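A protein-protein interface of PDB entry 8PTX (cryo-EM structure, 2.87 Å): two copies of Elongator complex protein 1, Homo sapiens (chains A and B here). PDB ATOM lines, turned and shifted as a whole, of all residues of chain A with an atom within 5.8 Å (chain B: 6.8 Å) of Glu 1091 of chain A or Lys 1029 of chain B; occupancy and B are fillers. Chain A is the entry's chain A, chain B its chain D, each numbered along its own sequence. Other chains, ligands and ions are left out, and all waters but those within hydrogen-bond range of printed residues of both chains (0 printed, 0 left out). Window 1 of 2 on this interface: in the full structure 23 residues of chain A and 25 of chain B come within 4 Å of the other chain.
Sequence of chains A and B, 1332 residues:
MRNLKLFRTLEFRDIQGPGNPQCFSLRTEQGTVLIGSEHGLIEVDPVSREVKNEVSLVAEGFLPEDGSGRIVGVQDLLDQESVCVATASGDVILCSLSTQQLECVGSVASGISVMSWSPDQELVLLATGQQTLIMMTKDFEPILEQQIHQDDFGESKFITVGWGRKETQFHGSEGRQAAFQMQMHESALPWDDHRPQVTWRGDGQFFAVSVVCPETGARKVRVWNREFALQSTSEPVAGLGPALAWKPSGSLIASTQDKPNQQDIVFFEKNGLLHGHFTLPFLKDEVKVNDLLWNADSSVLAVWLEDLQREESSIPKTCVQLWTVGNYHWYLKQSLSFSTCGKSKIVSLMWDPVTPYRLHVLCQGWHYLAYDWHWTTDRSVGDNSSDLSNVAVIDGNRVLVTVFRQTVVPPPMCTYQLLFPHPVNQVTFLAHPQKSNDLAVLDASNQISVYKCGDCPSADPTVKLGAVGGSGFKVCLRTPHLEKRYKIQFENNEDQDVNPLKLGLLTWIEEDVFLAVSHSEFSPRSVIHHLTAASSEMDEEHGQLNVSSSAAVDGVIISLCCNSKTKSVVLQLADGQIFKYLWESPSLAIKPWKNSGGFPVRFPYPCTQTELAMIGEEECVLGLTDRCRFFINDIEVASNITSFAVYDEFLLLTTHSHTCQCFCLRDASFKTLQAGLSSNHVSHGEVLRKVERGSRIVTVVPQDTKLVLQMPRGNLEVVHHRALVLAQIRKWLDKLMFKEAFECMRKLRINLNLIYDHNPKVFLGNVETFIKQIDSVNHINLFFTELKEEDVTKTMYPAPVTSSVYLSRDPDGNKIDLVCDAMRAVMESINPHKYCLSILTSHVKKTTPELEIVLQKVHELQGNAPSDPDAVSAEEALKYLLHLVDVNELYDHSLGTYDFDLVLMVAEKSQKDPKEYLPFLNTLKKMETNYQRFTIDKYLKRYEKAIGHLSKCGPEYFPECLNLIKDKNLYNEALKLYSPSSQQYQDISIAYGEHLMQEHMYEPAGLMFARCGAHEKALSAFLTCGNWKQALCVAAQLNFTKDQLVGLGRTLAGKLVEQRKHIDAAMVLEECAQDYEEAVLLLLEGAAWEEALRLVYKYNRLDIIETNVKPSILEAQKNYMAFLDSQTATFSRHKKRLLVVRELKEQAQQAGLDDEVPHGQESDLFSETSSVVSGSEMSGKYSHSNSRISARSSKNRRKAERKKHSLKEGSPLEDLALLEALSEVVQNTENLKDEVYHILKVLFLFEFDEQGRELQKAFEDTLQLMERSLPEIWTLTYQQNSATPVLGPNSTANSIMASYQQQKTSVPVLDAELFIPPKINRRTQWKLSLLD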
ATOM      1  N   ILE A1063     -13.292 -14.790 -21.481  1.00  0.00           N
ATOM      2  CA  ILE A1063     -13.787 -15.090 -20.141  1.00  0.00           C
ATOM      3  C   ILE A1063     -13.406 -16.510 -19.750  1.00  0.00           C
ATOM      4  O   ILE A1063     -12.928 -16.762 -18.638  1.00  0.00           O
ATOM      5  CB  ILE A1063     -15.312 -14.887 -20.073  1.00  0.00           C
ATOM      6  CG1 ILE A1063     -15.694 -13.483 -20.546  1.00  0.00           C
ATOM      7  CG2 ILE A1063     -15.815 -15.127 -18.660  1.00  0.00           C
ATOM      8  CD1 ILE A1063     -15.103 -12.374 -19.718  1.00  0.00           C
ATOM      9  N   VAL A1080      -6.663 -11.176 -15.279  1.00  0.00           N
ATOM     10  CA  VAL A1080      -7.181  -9.818 -15.390  1.00  0.00           C
ATOM     11  C   VAL A1080      -6.810  -9.215 -16.737  1.00  0.00           C
ATOM     12  O   VAL A1080      -7.587  -8.453 -17.313  1.00  0.00           O
ATOM     13  CB  VAL A1080      -6.708  -8.934 -14.219  1.00  0.00           C
ATOM     14  CG1 VAL A1080      -7.290  -9.429 -12.909  1.00  0.00           C
ATOM     15  CG2 VAL A1080      -5.195  -8.853 -14.150  1.00  0.00           C
ATOM     16  N   LEU A1083      -9.255 -10.617 -19.207  1.00  0.00           N
ATOM     17  CA  LEU A1083     -10.566 -10.033 -18.945  1.00  0.00           C
ATOM     18  C   LEU A1083     -10.638  -8.596 -19.447  1.00  0.00           C
ATOM     19  O   LEU A1083     -11.672  -8.168 -19.974  1.00  0.00           O
ATOM     20  CB  LEU A1083     -10.879 -10.103 -17.452  1.00  0.00           C
ATOM     21  CG  LEU A1083     -11.053 -11.529 -16.926  1.00  0.00           C
ATOM     22  CD1 LEU A1083     -11.117 -11.563 -15.409  1.00  0.00           C
ATOM     23  CD2 LEU A1083     -12.266 -12.198 -17.542  1.00  0.00           C
ATOM     24  N   ALA A1088     -14.789  -7.079 -20.512  1.00  0.00           N
ATOM     25  CA  ALA A1088     -15.474  -7.172 -19.224  1.00  0.00           C
ATOM     26  C   ALA A1088     -14.555  -6.653 -18.116  1.00  0.00           C
ATOM     27  O   ALA A1088     -13.516  -7.227 -17.797  1.00  0.00           O
ATOM     28  CB  ALA A1088     -15.927  -8.603 -18.966  1.00  0.00           C
ATOM     29  N   TRP A1089     -14.973  -5.532 -17.525  1.00  0.00           N
ATOM     30  CA  TRP A1089     -14.033  -4.700 -16.780  1.00  0.00           C
ATOM     31  C   TRP A1089     -14.245  -4.855 -15.279  1.00  0.00           C
ATOM     32  O   TRP A1089     -13.305  -4.737 -14.483  1.00  0.00           O
ATOM     33  CB  TRP A1089     -14.223  -3.245 -17.203  1.00  0.00           C
ATOM     34  CG  TRP A1089     -13.908  -3.011 -18.657  1.00  0.00           C
ATOM     35  CD1 TRP A1089     -14.814  -2.933 -19.674  1.00  0.00           C
ATOM     36  CD2 TRP A1089     -12.617  -2.853 -19.261  1.00  0.00           C
ATOM     37  NE1 TRP A1089     -14.174  -2.727 -20.868  1.00  0.00           N
ATOM     38  CE2 TRP A1089     -12.825  -2.673 -20.643  1.00  0.00           C
ATOM     39  CE3 TRP A1089     -11.310  -2.840 -18.770  1.00  0.00           C
ATOM     40  CZ2 TRP A1089     -11.777  -2.483 -21.537  1.00  0.00           C
ATOM     41  CZ3 TRP A1089     -10.272  -2.648 -19.664  1.00  0.00           C
ATOM     42  CH2 TRP A1089     -10.515  -2.476 -21.028  1.00  0.00           C
ATOM     43  N   GLU A1090     -15.490  -5.130 -14.878  1.00  0.00           N
ATOM     44  CA  GLU A1090     -15.858  -5.092 -13.468  1.00  0.00           C
ATOM     45  C   GLU A1090     -15.202  -6.224 -12.686  1.00  0.00           C
ATOM     46  O   GLU A1090     -14.674  -6.007 -11.589  1.00  0.00           O
ATOM     47  CB  GLU A1090     -17.377  -5.157 -13.342  1.00  0.00           C
ATOM     48  CG  GLU A1090     -18.076  -3.835 -13.614  1.00  0.00           C
ATOM     49  CD  GLU A1090     -19.543  -4.019 -13.939  1.00  0.00           C
ATOM     50  OE1 GLU A1090     -19.996  -5.183 -13.988  1.00  0.00           O
ATOM     51  OE2 GLU A1090     -20.243  -3.007 -14.146  1.00  0.00           O
ATOM     52  N   GLU A1091     -15.220  -7.441 -13.234  1.00  0.00           N
ATOM     53  CA  GLU A1091     -14.561  -8.552 -12.554  1.00  0.00           C
ATOM     54  C   GLU A1091     -13.048  -8.396 -12.593  1.00  0.00           C
ATOM     55  O   GLU A1091     -12.347  -8.857 -11.685  1.00  0.00           O
ATOM     56  CB  GLU A1091     -14.991  -9.881 -13.174  1.00  0.00           C
ATOM     57  CG  GLU A1091     -14.217 -10.289 -14.404  1.00  0.00           C
ATOM     58  CD  GLU A1091     -14.705  -9.596 -15.660  1.00  0.00           C
ATOM     59  OE1 GLU A1091     -15.445  -8.595 -15.553  1.00  0.00           O
ATOM     60  OE2 GLU A1091     -14.344 -10.052 -16.760  1.00  0.00           O
ATOM     61  N   ALA A1092     -12.523  -7.737 -13.629  1.00  0.00           N
ATOM     62  CA  ALA A1092     -11.102  -7.419 -13.638  1.00  0.00           C
ATOM     63  C   ALA A1092     -10.746  -6.516 -12.467  1.00  0.00           C
ATOM     64  O   ALA A1092      -9.773  -6.772 -11.748  1.00  0.00           O
ATOM     65  CB  ALA A1092     -10.718  -6.764 -14.963  1.00  0.00           C
ATOM     66  N   LEU A1093     -11.546  -5.471 -12.239  1.00  0.00           N
ATOM     67  CA  LEU A1093     -11.319  -4.601 -11.089  1.00  0.00           C
ATOM     68  C   LEU A1093     -11.500  -5.357  -9.777  1.00  0.00           C
ATOM     69  O   LEU A1093     -10.781  -5.108  -8.803  1.00  0.00           O
ATOM     70  CB  LEU A1093     -12.259  -3.397 -11.146  1.00  0.00           C
ATOM     71  CG  LEU A1093     -11.921  -2.234 -10.213  1.00  0.00           C
ATOM     72  CD1 LEU A1093     -10.743  -1.432 -10.746  1.00  0.00           C
ATOM     73  CD2 LEU A1093     -13.136  -1.342 -10.007  1.00  0.00           C
ATOM     74  N   ARG A1094     -12.471  -6.273  -9.730  1.00  0.00           N
ATOM     75  CA  ARG A1094     -12.694  -7.062  -8.523  1.00  0.00           C
ATOM     76  C   ARG A1094     -11.482  -7.925  -8.191  1.00  0.00           C
ATOM     77  O   ARG A1094     -11.064  -7.995  -7.030  1.00  0.00           O
ATOM     78  CB  ARG A1094     -13.944  -7.926  -8.690  1.00  0.00           C
ATOM     79  CG  ARG A1094     -14.455  -8.550  -7.403  1.00  0.00           C
ATOM     80  CD  ARG A1094     -15.570  -9.551  -7.679  1.00  0.00           C
ATOM     81  NE  ARG A1094     -15.088 -10.751  -8.354  1.00  0.00           N
ATOM     82  CZ  ARG A1094     -14.422 -11.733  -7.761  1.00  0.00           C
ATOM     83  NH1 ARG A1094     -14.131 -11.691  -6.472  1.00  0.00           N
ATOM     84  NH2 ARG A1094     -14.037 -12.783  -8.481  1.00  0.00           N
ATOM     85  N   LEU A1095     -10.899  -8.581  -9.196  1.00  0.00           N
ATOM     86  CA  LEU A1095      -9.697  -9.373  -8.962  1.00  0.00           C
ATOM     87  C   LEU A1095      -8.498  -8.493  -8.632  1.00  0.00           C
ATOM     88  O   LEU A1095      -7.637  -8.897  -7.841  1.00  0.00           O
ATOM     89  CB  LEU A1095      -9.393 -10.253 -10.174  1.00  0.00           C
ATOM     90  CG  LEU A1095      -9.991 -11.662 -10.194  1.00  0.00           C
ATOM     91  CD1 LEU A1095     -11.490 -11.625 -10.428  1.00  0.00           C
ATOM     92  CD2 LEU A1095      -9.304 -12.522 -11.242  1.00  0.00           C
ATOM     93  N   VAL A1096      -8.416  -7.301  -9.228  1.00  0.00           N
ATOM     94  CA  VAL A1096      -7.331  -6.378  -8.903  1.00  0.00           C
ATOM     95  C   VAL A1096      -7.401  -5.970  -7.437  1.00  0.00           C
ATOM     96  O   VAL A1096      -6.392  -5.979  -6.720  1.00  0.00           O
ATOM     97  CB  VAL A1096      -7.370  -5.152  -9.833  1.00  0.00           C
ATOM     98  CG1 VAL A1096      -6.423  -4.084  -9.335  1.00  0.00           C
ATOM     99  CG2 VAL A1096      -6.987  -5.552 -11.247  1.00  0.00           C
ATOM    100  N   HIS A1238     -22.090  -1.227 -20.935  1.00  0.00           N
ATOM    101  CA  HIS A1238     -21.040  -1.594 -19.987  1.00  0.00           C
ATOM    102  C   HIS A1238     -19.867  -0.621 -20.056  1.00  0.00           C
ATOM    103  O   HIS A1238     -19.308  -0.225 -19.024  1.00  0.00           O
ATOM    104  CB  HIS A1238     -20.565  -3.022 -20.247  1.00  0.00           C
ATOM    105  CG  HIS A1238     -19.635  -3.543 -19.196  1.00  0.00           C
ATOM    106  ND1 HIS A1238     -20.068  -3.935 -17.948  1.00  0.00           N
ATOM    107  CD2 HIS A1238     -18.294  -3.721 -19.202  1.00  0.00           C
ATOM    108  CE1 HIS A1238     -19.034  -4.341 -17.234  1.00  0.00           C
ATOM    109  NE2 HIS A1238     -17.944  -4.221 -17.971  1.00  0.00           N
ATOM    110  N   PHE B1022     -24.868  -1.101  -3.746  1.00  0.00           N
ATOM    111  CA  PHE B1022     -24.547  -2.268  -4.561  1.00  0.00           C
ATOM    112  C   PHE B1022     -25.201  -3.524  -3.998  1.00  0.00           C
ATOM    113  O   PHE B1022     -25.670  -4.384  -4.753  1.00  0.00           O
ATOM    114  CB  PHE B1022     -23.031  -2.441  -4.659  1.00  0.00           C
ATOM    115  CG  PHE B1022     -22.359  -1.420  -5.538  1.00  0.00           C
ATOM    116  CD1 PHE B1022     -22.946  -1.018  -6.728  1.00  0.00           C
ATOM    117  CD2 PHE B1022     -21.148  -0.856  -5.170  1.00  0.00           C
ATOM    118  CE1 PHE B1022     -22.333  -0.078  -7.536  1.00  0.00           C
ATOM    119  CE2 PHE B1022     -20.533   0.089  -5.972  1.00  0.00           C
ATOM    120  CZ  PHE B1022     -21.126   0.477  -7.158  1.00  0.00           C
ATOM    121  N   GLY B1026     -28.451  -5.718  -5.827  1.00  0.00           N
ATOM    122  CA  GLY B1026     -28.032  -7.059  -6.165  1.00  0.00           C
ATOM    123  C   GLY B1026     -26.677  -7.160  -6.824  1.00  0.00           C
ATOM    124  O   GLY B1026     -26.266  -8.269  -7.190  1.00  0.00           O
ATOM    125  N   ASN B1027     -25.965  -6.045  -6.984  1.00  0.00           N
ATOM    126  CA  ASN B1027     -24.649  -6.048  -7.621  1.00  0.00           C
ATOM    127  C   ASN B1027     -23.622  -6.572  -6.621  1.00  0.00           C
ATOM    128  O   ASN B1027     -22.962  -5.821  -5.897  1.00  0.00           O
ATOM    129  CB  ASN B1027     -24.283  -4.657  -8.121  1.00  0.00           C
ATOM    130  CG  ASN B1027     -23.630  -4.683  -9.486  1.00  0.00           C
ATOM    131  OD1 ASN B1027     -22.804  -5.549  -9.775  1.00  0.00           O
ATOM    132  ND2 ASN B1027     -23.993  -3.730 -10.336  1.00  0.00           N
ATOM    133  N   TRP B1028     -23.497  -7.900  -6.583  1.00  0.00           N
ATOM    134  CA  TRP B1028     -22.455  -8.535  -5.784  1.00  0.00           C
ATOM    135  C   TRP B1028     -21.073  -8.094  -6.243  1.00  0.00           C
ATOM    136  O   TRP B1028     -20.119  -8.077  -5.456  1.00  0.00           O
ATOM    137  CB  TRP B1028     -22.575 -10.054  -5.897  1.00  0.00           C
ATOM    138  CG  TRP B1028     -22.102 -10.566  -7.229  1.00  0.00           C
ATOM    139  CD1 TRP B1028     -20.931 -11.220  -7.483  1.00  0.00           C
ATOM    140  CD2 TRP B1028     -22.765 -10.429  -8.494  1.00  0.00           C
ATOM    141  NE1 TRP B1028     -20.834 -11.516  -8.820  1.00  0.00           N
ATOM    142  CE2 TRP B1028     -21.946 -11.040  -9.463  1.00  0.00           C
ATOM    143  CE3 TRP B1028     -23.975  -9.858  -8.899  1.00  0.00           C
ATOM    144  CZ2 TRP B1028     -22.297 -11.096 -10.809  1.00  0.00           C
ATOM    145  CZ3 TRP B1028     -24.322  -9.916 -10.236  1.00  0.00           C
ATOM    146  CH2 TRP B1028     -23.486 -10.530 -11.174  1.00  0.00           C
ATOM    147  N   LYS B1029     -20.956  -7.715  -7.514  1.00  0.00           N
ATOM    148  CA  LYS B1029     -19.654  -7.498  -8.133  1.00  0.00           C
ATOM    149  C   LYS B1029     -18.996  -6.235  -7.595  1.00  0.00           C
ATOM    150  O   LYS B1029     -17.896  -6.277  -7.026  1.00  0.00           O
ATOM    151  CB  LYS B1029     -19.850  -7.413  -9.645  1.00  0.00           C
ATOM    152  CG  LYS B1029     -18.677  -7.809 -10.502  1.00  0.00           C
ATOM    153  CD  LYS B1029     -19.180  -7.977 -11.928  1.00  0.00           C
ATOM    154  CE  LYS B1029     -18.241  -8.802 -12.766  1.00  0.00           C
ATOM    155  NZ  LYS B1029     -18.063 -10.160 -12.183  1.00  0.00           N
ATOM    156  N   GLN B1030     -19.665  -5.095  -7.754  1.00  0.00           N
ATOM    157  CA  GLN B1030     -19.108  -3.840  -7.263  1.00  0.00           C
ATOM    158  C   GLN B1030     -19.150  -3.778  -5.744  1.00  0.00           C
ATOM    159  O   GLN B1030     -18.334  -3.090  -5.122  1.00  0.00           O
ATOM    160  CB  GLN B1030     -19.851  -2.661  -7.885  1.00  0.00           C
ATOM    161  CG  GLN B1030     -19.413  -2.363  -9.303  1.00  0.00           C
ATOM    162  CD  GLN B1030     -19.662  -3.528 -10.230  1.00  0.00           C
ATOM    163  OE1 GLN B1030     -18.726  -4.184 -10.678  1.00  0.00           O
ATOM    164  NE2 GLN B1030     -20.927  -3.793 -10.524  1.00  0.00           N
ATOM    165  N   ALA B1031     -20.087  -4.501  -5.126  1.00  0.00           N
ATOM    166  CA  ALA B1031     -20.059  -4.635  -3.675  1.00  0.00           C
ATOM    167  C   ALA B1031     -18.774  -5.313  -3.218  1.00  0.00           C
ATOM    168  O   ALA B1031     -18.130  -4.863  -2.264  1.00  0.00           O
ATOM    169  CB  ALA B1031     -21.281  -5.416  -3.194  1.00  0.00           C
ATOM    170  N   LEU B1032     -18.379  -6.390  -3.901  1.00  0.00           N
ATOM    171  CA  LEU B1032     -17.111  -7.044  -3.594  1.00  0.00           C
ATOM    172  C   LEU B1032     -15.934  -6.120  -3.874  1.00  0.00           C
ATOM    173  O   LEU B1032     -14.949  -6.120  -3.129  1.00  0.00           O
ATOM    174  CB  LEU B1032     -16.979  -8.337  -4.398  1.00  0.00           C
ATOM    175  CG  LEU B1032     -17.702  -9.562  -3.836  1.00  0.00           C
ATOM    176  CD1 LEU B1032     -17.891 -10.614  -4.917  1.00  0.00           C
ATOM    177  CD2 LEU B1032     -16.942 -10.134  -2.649  1.00  0.00           C
ATOM    178  N   CYS B1033     -16.014  -5.339  -4.954  1.00  0.00           N
ATOM    179  CA  CYS B1033     -14.955  -4.378  -5.254  1.00  0.00           C
ATOM    180  C   CYS B1033     -14.773  -3.387  -4.107  1.00  0.00           C
ATOM    181  O   CYS B1033     -13.650  -3.137  -3.652  1.00  0.00           O
ATOM    182  CB  CYS B1033     -15.274  -3.635  -6.553  1.00  0.00           C
ATOM    183  SG  CYS B1033     -15.282  -4.662  -8.036  1.00  0.00           S
ATOM    184  N   VAL B1034     -15.881  -2.821  -3.623  1.00  0.00           N
ATOM    185  CA  VAL B1034     -15.820  -1.852  -2.531  1.00  0.00           C
ATOM    186  C   VAL B1034     -15.329  -2.517  -1.250  1.00  0.00           C
ATOM    187  O   VAL B1034     -14.537  -1.938  -0.497  1.00  0.00           O
ATOM    188  CB  VAL B1034     -17.192  -1.181  -2.336  1.00  0.00           C
ATOM    189  CG1 VAL B1034     -17.182  -0.296  -1.100  1.00  0.00           C
ATOM    190  CG2 VAL B1034     -17.565  -0.369  -3.567  1.00  0.00           C
ATOM    191  N   LEU B1052     -25.101 -12.495  -0.130  1.00  0.00           N
ATOM    192  CA  LEU B1052     -25.133 -12.004  -1.505  1.00  0.00           C
ATOM    193  C   LEU B1052     -25.550 -13.106  -2.469  1.00  0.00           C
ATOM    194  O   LEU B1052     -26.329 -12.866  -3.399  1.00  0.00           O
ATOM    195  CB  LEU B1052     -23.767 -11.444  -1.897  1.00  0.00           C
ATOM    196  CG  LEU B1052     -23.601  -9.931  -1.773  1.00  0.00           C
ATOM    197  CD1 LEU B1052     -22.140  -9.540  -1.945  1.00  0.00           C
ATOM    198  CD2 LEU B1052     -24.477  -9.221  -2.790  1.00  0.00           C
ATOM    199  N   MET B1067     -20.892 -19.217  -7.722  1.00  0.00           N
ATOM    200  CA  MET B1067     -19.567 -18.618  -7.845  1.00  0.00           C
ATOM    201  C   MET B1067     -19.218 -17.794  -6.613  1.00  0.00           C
ATOM    202  O   MET B1067     -18.090 -17.863  -6.112  1.00  0.00           O
ATOM    203  CB  MET B1067     -19.492 -17.755  -9.105  1.00  0.00           C
ATOM    204  CG  MET B1067     -19.514 -18.544 -10.404  1.00  0.00           C
ATOM    205  SD  MET B1067     -18.393 -17.864 -11.643  1.00  0.00           S
ATOM    206  CE  MET B1067     -19.418 -16.587 -12.366  1.00  0.00           C
ATOM    207  N   VAL B1068     -20.175 -17.012  -6.106  1.00  0.00           N
ATOM    208  CA  VAL B1068     -19.913 -16.199  -4.921  1.00  0.00           C
ATOM    209  C   VAL B1068     -19.647 -17.082  -3.710  1.00  0.00           C
ATOM    210  O   VAL B1068     -18.726 -16.818  -2.927  1.00  0.00           O
ATOM    211  CB  VAL B1068     -21.072 -15.221  -4.668  1.00  0.00           C
ATOM    212  CG1 VAL B1068     -20.839 -14.455  -3.379  1.00  0.00           C
ATOM    213  CG2 VAL B1068     -21.199 -14.251  -5.825  1.00  0.00           C
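N of Arg 1094 of chain A sits close to SG of Cys 1033 of chain B, at 3.7 Å.
The side-chain amide oxygen (OD1) of Asn 1027 of chain B sits at hydrogen-bond distance from the side-chain amide nitrogen (NE2) of Gln 1030 of chain B (2.7 Å).
O of Lys 1029 of chain B is in hydrogen-bond range of SG of Cys 1033 of chain B, 3.2 Å away.
Among the printed residues, merely in contact across the chains: Glu 1090 of chain A with Gln 1030 of chain B (3.0 Å), Glu 1091 of chain A with Lys 1029 of chain B (3.2 Å), Glu 1090 of chain A with Lys 1029 of chain B (3.6 Å), Arg 1094 of chain A with Leu 1032 of chain B (3.8 Å) and Glu 1090 of chain A with Cys 1033 of chain B (3.8 Å).
Glu 1091 of chain A touches just one residue of chain B: Lys 1029 (3.2 Å).
Of the printed residues of chain A, Lys 1029 of chain B touches Glu 1090 (3.6 Å) and Glu 1091 (3.2 Å).
Of the printed residues of chain A, Gln 1030 of chain B touches Glu 1090 (3.0 Å).
Of the printed residues of chain B, Arg 1094 of chain A touches Leu 1032 (3.8 Å) and Cys 1033 (3.6 Å).
Ala 1092 of chain A touches none of the printed residues of chain B.
Phe 1022 of chain B touches none of the printed residues of chain A.
The nearest printed residue of chain A that does not touch Gln 1030 of chain B is Glu 1091 of chain A (5.4 Å).
Of the 13 printed residues of chain A, 3 touch a printed residue of chain B.
Of the 13 printed residues of chain B, 4 touch a printed residue of chain A.
Hydrophobic or aromatic side chains of chain B within 4 Å of the printed part of chain A: Leu 1032.
Among the printed residues, no Asp or Glu carboxylate lies within 4 Å of a Lys or Arg side-chain nitrogen of the other chain.
No position is printed for both chains.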
